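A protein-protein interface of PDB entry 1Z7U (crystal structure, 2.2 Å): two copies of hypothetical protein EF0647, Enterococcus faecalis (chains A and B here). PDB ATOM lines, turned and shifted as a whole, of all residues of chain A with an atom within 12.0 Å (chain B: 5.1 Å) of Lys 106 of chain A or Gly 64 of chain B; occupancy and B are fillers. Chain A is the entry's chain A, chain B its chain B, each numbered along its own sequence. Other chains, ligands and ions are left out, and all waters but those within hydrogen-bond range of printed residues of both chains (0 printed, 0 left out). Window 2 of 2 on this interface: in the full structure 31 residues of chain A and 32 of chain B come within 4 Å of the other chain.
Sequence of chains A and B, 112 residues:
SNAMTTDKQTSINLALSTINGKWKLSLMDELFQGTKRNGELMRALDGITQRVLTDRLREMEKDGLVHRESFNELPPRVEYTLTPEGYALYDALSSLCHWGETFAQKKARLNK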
ATOM      1  N   CYS A  97      11.534 -26.439  -0.540  1.00  0.00           N
ATOM      2  CA  CYS A  97      11.169 -25.162   0.010  1.00  0.00           C
ATOM      3  C   CYS A  97      12.432 -24.392   0.391  1.00  0.00           C
ATOM      4  O   CYS A  97      12.559 -23.227   0.074  1.00  0.00           O
ATOM      5  CB  CYS A  97      10.258 -25.346   1.219  1.00  0.00           C
ATOM      6  SG  CYS A  97       9.880 -23.810   2.006  1.00  0.00           S
ATOM      7  N   HIS A  98      13.357 -25.069   1.070  1.00  0.00           N
ATOM      8  CA  HIS A  98      14.594 -24.472   1.545  1.00  0.00           C
ATOM      9  C   HIS A  98      15.436 -24.013   0.346  1.00  0.00           C
ATOM     10  O   HIS A  98      15.945 -22.898   0.324  1.00  0.00           O
ATOM     11  CB  HIS A  98      15.347 -25.495   2.411  1.00  0.00           C
ATOM     12  CG  HIS A  98      16.426 -24.909   3.272  1.00  0.00           C
ATOM     13  ND1 HIS A  98      17.227 -23.864   2.867  1.00  0.00           N
ATOM     14  CD2 HIS A  98      16.879 -25.270   4.495  1.00  0.00           C
ATOM     15  CE1 HIS A  98      18.103 -23.583   3.814  1.00  0.00           C
ATOM     16  NE2 HIS A  98      17.916 -24.425   4.813  1.00  0.00           N
ATOM     17  N   TRP A  99      15.545 -24.859  -0.671  1.00  0.00           N
ATOM     18  CA  TRP A  99      16.169 -24.448  -1.915  1.00  0.00           C
ATOM     19  C   TRP A  99      15.560 -23.163  -2.521  1.00  0.00           C
ATOM     20  O   TRP A  99      16.295 -22.210  -2.842  1.00  0.00           O
ATOM     21  CB  TRP A  99      16.160 -25.586  -2.949  1.00  0.00           C
ATOM     22  CG  TRP A  99      17.195 -25.342  -3.951  1.00  0.00           C
ATOM     23  CD1 TRP A  99      18.488 -25.754  -3.898  1.00  0.00           C
ATOM     24  CD2 TRP A  99      17.069 -24.540  -5.138  1.00  0.00           C
ATOM     25  NE1 TRP A  99      19.174 -25.288  -4.996  1.00  0.00           N
ATOM     26  CE2 TRP A  99      18.323 -24.539  -5.770  1.00  0.00           C
ATOM     27  CE3 TRP A  99      16.017 -23.834  -5.727  1.00  0.00           C
ATOM     28  CZ2 TRP A  99      18.554 -23.855  -6.954  1.00  0.00           C
ATOM     29  CZ3 TRP A  99      16.244 -23.166  -6.920  1.00  0.00           C
ATOM     30  CH2 TRP A  99      17.501 -23.177  -7.513  1.00  0.00           C
ATOM     31  N   GLY A 100      14.239 -23.143  -2.703  1.00  0.00           N
ATOM     32  CA  GLY A 100      13.580 -21.986  -3.318  1.00  0.00           C
ATOM     33  C   GLY A 100      13.687 -20.699  -2.514  1.00  0.00           C
ATOM     34  O   GLY A 100      13.682 -19.611  -3.062  1.00  0.00           O
ATOM     35  N   GLU A 101      13.771 -20.827  -1.200  1.00  0.00           N
ATOM     36  CA  GLU A 101      13.953 -19.704  -0.291  1.00  0.00           C
ATOM     37  C   GLU A 101      15.343 -19.090  -0.497  1.00  0.00           C
ATOM     38  O   GLU A 101      15.481 -17.887  -0.657  1.00  0.00           O
ATOM     39  CB  GLU A 101      13.786 -20.227   1.145  1.00  0.00           C
ATOM     40  CG  GLU A 101      13.873 -19.205   2.251  1.00  0.00           C
ATOM     41  CD  GLU A 101      13.896 -19.861   3.629  1.00  0.00           C
ATOM     42  OE1 GLU A 101      12.836 -19.883   4.300  1.00  0.00           O
ATOM     43  OE2 GLU A 101      14.973 -20.382   4.028  1.00  0.00           O
ATOM     44  N   THR A 102      16.370 -19.932  -0.498  1.00  0.00           N
ATOM     45  CA  THR A 102      17.738 -19.483  -0.720  1.00  0.00           C
ATOM     46  C   THR A 102      17.881 -18.798  -2.085  1.00  0.00           C
ATOM     47  O   THR A 102      18.395 -17.691  -2.185  1.00  0.00           O
ATOM     48  CB  THR A 102      18.702 -20.663  -0.596  1.00  0.00           C
ATOM     49  OG1 THR A 102      18.544 -21.220   0.708  1.00  0.00           O
ATOM     50  CG2 THR A 102      20.169 -20.210  -0.772  1.00  0.00           C
ATOM     51  N   PHE A 103      17.377 -19.463  -3.122  1.00  0.00           N
ATOM     52  CA  PHE A 103      17.404 -18.948  -4.482  1.00  0.00           C
ATOM     53  C   PHE A 103      16.678 -17.613  -4.636  1.00  0.00           C
ATOM     54  O   PHE A 103      17.229 -16.681  -5.224  1.00  0.00           O
ATOM     55  CB  PHE A 103      16.839 -20.004  -5.427  1.00  0.00           C
ATOM     56  CG  PHE A 103      16.817 -19.599  -6.856  1.00  0.00           C
ATOM     57  CD1 PHE A 103      17.991 -19.514  -7.591  1.00  0.00           C
ATOM     58  CD2 PHE A 103      15.613 -19.319  -7.480  1.00  0.00           C
ATOM     59  CE1 PHE A 103      17.958 -19.139  -8.935  1.00  0.00           C
ATOM     60  CE2 PHE A 103      15.574 -18.960  -8.802  1.00  0.00           C
ATOM     61  CZ  PHE A 103      16.747 -18.870  -9.538  1.00  0.00           C
ATOM     62  N   ALA A 104      15.458 -17.507  -4.100  1.00  0.00           N
ATOM     63  CA  ALA A 104      14.701 -16.254  -4.190  1.00  0.00           C
ATOM     64  C   ALA A 104      15.400 -15.088  -3.499  1.00  0.00           C
ATOM     65  O   ALA A 104      15.320 -13.952  -3.957  1.00  0.00           O
ATOM     66  CB  ALA A 104      13.284 -16.419  -3.650  1.00  0.00           C
ATOM     67  N   GLN A 105      16.072 -15.376  -2.396  1.00  0.00           N
ATOM     68  CA  GLN A 105      16.824 -14.354  -1.677  1.00  0.00           C
ATOM     69  C   GLN A 105      18.069 -13.882  -2.431  1.00  0.00           C
ATOM     70  O   GLN A 105      18.402 -12.701  -2.394  1.00  0.00           O
ATOM     71  CB  GLN A 105      17.132 -14.815  -0.250  1.00  0.00           C
ATOM     72  CG  GLN A 105      15.928 -14.619   0.671  1.00  0.00           C
ATOM     73  CD  GLN A 105      15.992 -15.430   1.946  1.00  0.00           C
ATOM     74  OE1 GLN A 105      17.063 -15.632   2.518  1.00  0.00           O
ATOM     75  NE2 GLN A 105      14.833 -15.896   2.406  1.00  0.00           N
ATOM     76  N   LYS A 106      18.747 -14.800  -3.111  1.00  0.00           N
ATOM     77  CA  LYS A 106      19.850 -14.450  -3.991  1.00  0.00           C
ATOM     78  C   LYS A 106      19.371 -13.524  -5.111  1.00  0.00           C
ATOM     79  O   LYS A 106      20.038 -12.526  -5.419  1.00  0.00           O
ATOM     80  CB  LYS A 106      20.474 -15.712  -4.581  1.00  0.00           C
ATOM     81  CG  LYS A 106      21.658 -15.486  -5.530  1.00  0.00           C
ATOM     82  CD  LYS A 106      21.643 -16.520  -6.662  1.00  0.00           C
ATOM     83  CE  LYS A 106      23.036 -16.777  -7.233  1.00  0.00           C
ATOM     84  NZ  LYS A 106      22.977 -17.748  -8.378  1.00  0.00           N
ATOM     85  N   LYS A 107      18.227 -13.858  -5.717  1.00  0.00           N
ATOM     86  CA  LYS A 107      17.660 -13.052  -6.803  1.00  0.00           C
ATOM     87  C   LYS A 107      17.335 -11.639  -6.344  1.00  0.00           C
ATOM     88  O   LYS A 107      17.610 -10.677  -7.057  1.00  0.00           O
ATOM     89  CB  LYS A 107      16.402 -13.693  -7.389  1.00  0.00           C
ATOM     90  CG  LYS A 107      16.660 -14.884  -8.286  1.00  0.00           C
ATOM     91  CD  LYS A 107      15.347 -15.444  -8.863  1.00  0.00           C
ATOM     92  CE  LYS A 107      15.038 -14.898 -10.263  1.00  0.00           C
ATOM     93  NZ  LYS A 107      13.910 -15.663 -10.906  1.00  0.00           N
ATOM     94  N   ALA A 108      16.751 -11.520  -5.156  1.00  0.00           N
ATOM     95  CA  ALA A 108      16.396 -10.222  -4.595  1.00  0.00           C
ATOM     96  C   ALA A 108      17.654  -9.384  -4.327  1.00  0.00           C
ATOM     97  O   ALA A 108      17.701  -8.191  -4.644  1.00  0.00           O
ATOM     98  CB  ALA A 108      15.576 -10.411  -3.327  1.00  0.00           C
ATOM     99  N   ARG A 109      18.673 -10.034  -3.768  1.00  0.00           N
ATOM    100  CA  ARG A 109      19.945  -9.401  -3.426  1.00  0.00           C
ATOM    101  C   ARG A 109      20.706  -8.878  -4.655  1.00  0.00           C
ATOM    102  O   ARG A 109      21.286  -7.793  -4.608  1.00  0.00           O
ATOM    103  CB  ARG A 109      20.809 -10.390  -2.638  1.00  0.00           C
ATOM    104  CG  ARG A 109      21.966  -9.779  -1.874  1.00  0.00           C
ATOM    105  CD  ARG A 109      22.443 -10.729  -0.777  1.00  0.00           C
ATOM    106  NE  ARG A 109      23.539 -10.173   0.026  1.00  0.00           N
ATOM    107  CZ  ARG A 109      23.391  -9.310   1.032  1.00  0.00           C
ATOM    108  NH1 ARG A 109      22.182  -8.867   1.382  1.00  0.00           N
ATOM    109  NH2 ARG A 109      24.460  -8.885   1.688  1.00  0.00           N
ATOM    110  N   LEU A 110      20.689  -9.645  -5.744  1.00  0.00           N
ATOM    111  CA  LEU A 110      21.435  -9.297  -6.961  1.00  0.00           C
ATOM    112  C   LEU A 110      20.634  -8.496  -7.995  1.00  0.00           C
ATOM    113  O   LEU A 110      21.182  -8.073  -9.018  1.00  0.00           O
ATOM    114  CB  LEU A 110      22.042 -10.554  -7.603  1.00  0.00           C
ATOM    115  CG  LEU A 110      22.989 -11.417  -6.757  1.00  0.00           C
ATOM    116  CD1 LEU A 110      23.560 -12.549  -7.599  1.00  0.00           C
ATOM    117  CD2 LEU A 110      24.121 -10.602  -6.108  1.00  0.00           C
ATOM    118  N   ASN A 111      19.350  -8.285  -7.726  1.00  0.00           N
ATOM    119  CA  ASN A 111      18.490  -7.511  -8.614  1.00  0.00           C
ATOM    120  C   ASN A 111      18.532  -6.012  -8.299  1.00  0.00           C
ATOM    121  O   ASN A 111      18.032  -5.556  -7.262  1.00  0.00           O
ATOM    122  CB  ASN A 111      17.057  -8.043  -8.557  1.00  0.00           C
ATOM    123  CG  ASN A 111      16.033  -7.010  -8.973  1.00  0.00           C
ATOM    124  OD1 ASN A 111      15.912  -6.675 -10.155  1.00  0.00           O
ATOM    125  ND2 ASN A 111      15.285  -6.495  -7.997  1.00  0.00           N
ATOM    126  N   MET B  60      20.422 -22.579 -16.945  1.00  0.00           N
ATOM    127  CA  MET B  60      20.837 -23.268 -15.714  1.00  0.00           C
ATOM    128  C   MET B  60      22.044 -22.602 -15.059  1.00  0.00           C
ATOM    129  O   MET B  60      22.138 -22.547 -13.840  1.00  0.00           O
ATOM    130  CB  MET B  60      21.119 -24.732 -15.994  1.00  0.00           C
ATOM    131  CG  MET B  60      19.904 -25.485 -16.425  1.00  0.00           C
ATOM    132  SD  MET B  60      20.319 -27.274 -17.069  1.00  0.00           S
ATOM    133  CE  MET B  60      20.450 -28.252 -15.231  1.00  0.00           C
ATOM    134  N   GLU B  61      22.955 -22.084 -15.879  1.00  0.00           N
ATOM    135  CA  GLU B  61      24.057 -21.261 -15.379  1.00  0.00           C
ATOM    136  C   GLU B  61      23.589 -19.935 -14.739  1.00  0.00           C
ATOM    137  O   GLU B  61      24.065 -19.565 -13.659  1.00  0.00           O
ATOM    138  CB  GLU B  61      25.102 -21.003 -16.472  1.00  0.00           C
ATOM    139  CG  GLU B  61      26.297 -20.190 -15.985  1.00  0.00           C
ATOM    140  CD  GLU B  61      27.331 -19.888 -17.078  1.00  0.00           C
ATOM    141  OE1 GLU B  61      27.151 -20.338 -18.237  1.00  0.00           O
ATOM    142  OE2 GLU B  61      28.326 -19.194 -16.763  1.00  0.00           O
ATOM    143  N   LYS B  62      22.667 -19.239 -15.405  1.00  0.00           N
ATOM    144  CA  LYS B  62      22.106 -17.994 -14.867  1.00  0.00           C
ATOM    145  C   LYS B  62      21.373 -18.245 -13.539  1.00  0.00           C
ATOM    146  O   LYS B  62      21.433 -17.414 -12.625  1.00  0.00           O
ATOM    147  CB  LYS B  62      21.156 -17.312 -15.869  1.00  0.00           C
ATOM    148  CG  LYS B  62      21.494 -17.482 -17.361  1.00  0.00           C
ATOM    149  CD  LYS B  62      22.348 -16.343 -17.956  1.00  0.00           C
ATOM    150  CE  LYS B  62      23.811 -16.756 -18.188  1.00  0.00           C
ATOM    151  NZ  LYS B  62      23.925 -18.041 -18.949  1.00  0.00           N
ATOM    152  N   ASP B  63      20.697 -19.391 -13.439  1.00  0.00           N
ATOM    153  CA  ASP B  63      19.985 -19.782 -12.215  1.00  0.00           C
ATOM    154  C   ASP B  63      20.911 -20.364 -11.138  1.00  0.00           C
ATOM    155  O   ASP B  63      20.423 -20.838 -10.109  1.00  0.00           O
ATOM    156  CB  ASP B  63      18.866 -20.773 -12.538  1.00  0.00           C
ATOM    157  CG  ASP B  63      17.665 -20.115 -13.218  1.00  0.00           C
ATOM    158  OD1 ASP B  63      17.553 -18.872 -13.229  1.00  0.00           O
ATOM    159  OD2 ASP B  63      16.812 -20.859 -13.739  1.00  0.00           O
ATOM    160  N   GLY B  64      22.233 -20.320 -11.382  1.00  0.00           N
ATOM    161  CA  GLY B  64      23.254 -20.845 -10.467  1.00  0.00           C
ATOM    162  C   GLY B  64      23.279 -22.350 -10.245  1.00  0.00           C
ATOM    163  O   GLY B  64      23.794 -22.816  -9.231  1.00  0.00           O
ATOM    164  N   LEU B  65      22.731 -23.121 -11.186  1.00  0.00           N
ATOM    165  CA  LEU B  65      22.690 -24.575 -11.050  1.00  0.00           C
ATOM    166  C   LEU B  65      23.905 -25.240 -11.698  1.00  0.00           C
ATOM    167  O   LEU B  65      24.305 -26.338 -11.302  1.00  0.00           O
ATOM    168  CB  LEU B  65      21.426 -25.154 -11.689  1.00  0.00           C
ATOM    169  CG  LEU B  65      20.044 -24.747 -11.188  1.00  0.00           C
ATOM    170  CD1 LEU B  65      18.987 -25.360 -12.101  1.00  0.00           C
ATOM    171  CD2 LEU B  65      19.852 -25.208  -9.762  1.00  0.00           C
ATOM    172  N   VAL B  66      24.453 -24.578 -12.714  1.00  0.00           N
ATOM    173  CA  VAL B  66      25.507 -25.152 -13.537  1.00  0.00           C
ATOM    174  C   VAL B  66      26.721 -24.215 -13.539  1.00  0.00           C
ATOM    175  O   VAL B  66      26.577 -22.997 -13.609  1.00  0.00           O
ATOM    176  CB  VAL B  66      24.981 -25.461 -14.979  1.00  0.00           C
ATOM    177  CG1 VAL B  66      26.108 -25.605 -15.999  1.00  0.00           C
ATOM    178  CG2 VAL B  66      24.119 -26.707 -14.977  1.00  0.00           C
ATOM    179  N   THR B  83      26.857 -26.906  -9.715  1.00  0.00           N
ATOM    180  CA  THR B  83      27.335 -26.133  -8.567  1.00  0.00           C
ATOM    181  C   THR B  83      26.883 -26.803  -7.243  1.00  0.00           C
ATOM    182  O   THR B  83      26.087 -27.762  -7.268  1.00  0.00           O
ATOM    183  CB  THR B  83      26.758 -24.734  -8.618  1.00  0.00           C
ATOM    184  OG1 THR B  83      25.333 -24.822  -8.489  1.00  0.00           O
ATOM    185  CG2 THR B  83      27.102 -24.072  -9.938  1.00  0.00           C
ATOM    186  N   GLU B  85      24.731 -25.521  -5.234  1.00  0.00           N
ATOM    187  CA  GLU B  85      23.295 -25.239  -5.295  1.00  0.00           C
ATOM    188  C   GLU B  85      22.590 -26.247  -6.205  1.00  0.00           C
ATOM    189  O   GLU B  85      21.517 -26.765  -5.873  1.00  0.00           O
ATOM    190  CB  GLU B  85      23.048 -23.810  -5.809  1.00  0.00           C
ATOM    191  CG  GLU B  85      23.498 -22.669  -4.875  1.00  0.00           C
ATOM    192  CD  GLU B  85      25.011 -22.590  -4.687  1.00  0.00           C
ATOM    193  OE1 GLU B  85      25.765 -22.748  -5.673  1.00  0.00           O
ATOM    194  OE2 GLU B  85      25.450 -22.364  -3.540  1.00  0.00           O
ATOM    195  N   GLY B  86      23.215 -26.524  -7.347  1.00  0.00           N
ATOM    196  CA  GLY B  86      22.742 -27.507  -8.305  1.00  0.00           C
ATOM    197  C   GLY B  86      22.615 -28.880  -7.672  1.00  0.00           C
ATOM    198  O   GLY B  86      21.591 -29.565  -7.847  1.00  0.00           O
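NE1 of Trp 99 of chain A is in hydrogen-bond range of O of Glu 85 of chain B.
The backbone carbonyl oxygen of Met 60 of chain B lies within hydrogen-bond range of the backbone NH of Leu 65 of chain B (2.8 Å). OG1 of Thr 83 of chain B lies within hydrogen-bond range of O of Gly 64 of chain B (2.6 Å). N of Thr 83 of chain B lies within hydrogen-bond range of O of Leu 65 of chain B (3.1 Å). The side-chain hydroxyl of Thr 83 of chain B lies close to the backbone NH of Glu 85 of chain B (3.4 Å).
Among the printed residues, pairs that only touch across the chains: Trp 99 of chain A with Leu 65 of chain B, Phe 103 of chain A with Asp 63 of chain B and Lys 106 of chain A with Gly 64 of chain B.
Of the printed residues of chain B, Trp 99 of chain A touches Leu 65 and Glu 85. Of the printed residues of chain B, Phe 103 of chain A touches Asp 63 (3.2 Å). Of chain B, only Gly 64 (3.7 Å) comes within 4 Å of Lys 106 of chain A. Lys 62 of chain B touches none of the printed residues of chain A. Asp 63 of chain B touches just one residue of chain A: Phe 103. Of chain A, only Lys 106 (3.7 Å) comes within 4 Å of Gly 64 of chain B. Of chain A, only Trp 99 (3.4 Å) comes within 4 Å of Leu 65 of chain B. No residue of chain A comes within 4 Å of Thr 83 of chain B. Of the printed residues of chain A, Glu 85 of chain B touches Trp 99 (2.9 Å). The nearest residue of chain B that does not touch Lys 106 of chain A is Asp 63 of chain B (4.3 Å). The nearest residue of chain A that does not touch Gly 64 of chain B is Phe 103 of chain A (5.1 Å).
Printed residues of chain A that touch a printed residue of chain B: Trp 99, Phe 103 and Lys 106. Hydrophobic or aromatic side chains of chain A that line the printed part of chain B: Trp 99 and Phe 103. Of the 10 printed residues of chain B, 4 touch a printed residue of chain A. Printed residues of chain B that touch a printed residue of chain A: Asp 63, Gly 64, Leu 65 and Glu 85. Hydrophobic or aromatic side chains of chain B within 4 Å of the printed part of chain A: Leu 65. Among the printed residues, 4 pairs touch across the chains. Among the printed residues, no Asp or Glu carboxylate lies within 4 Å of a Lys or Arg side-chain nitrogen of the other chain.
No position is printed for both chains. Of the 4 pairs that touch across the chains among the printed residues, none has its exchanged pair printed and touching as well.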
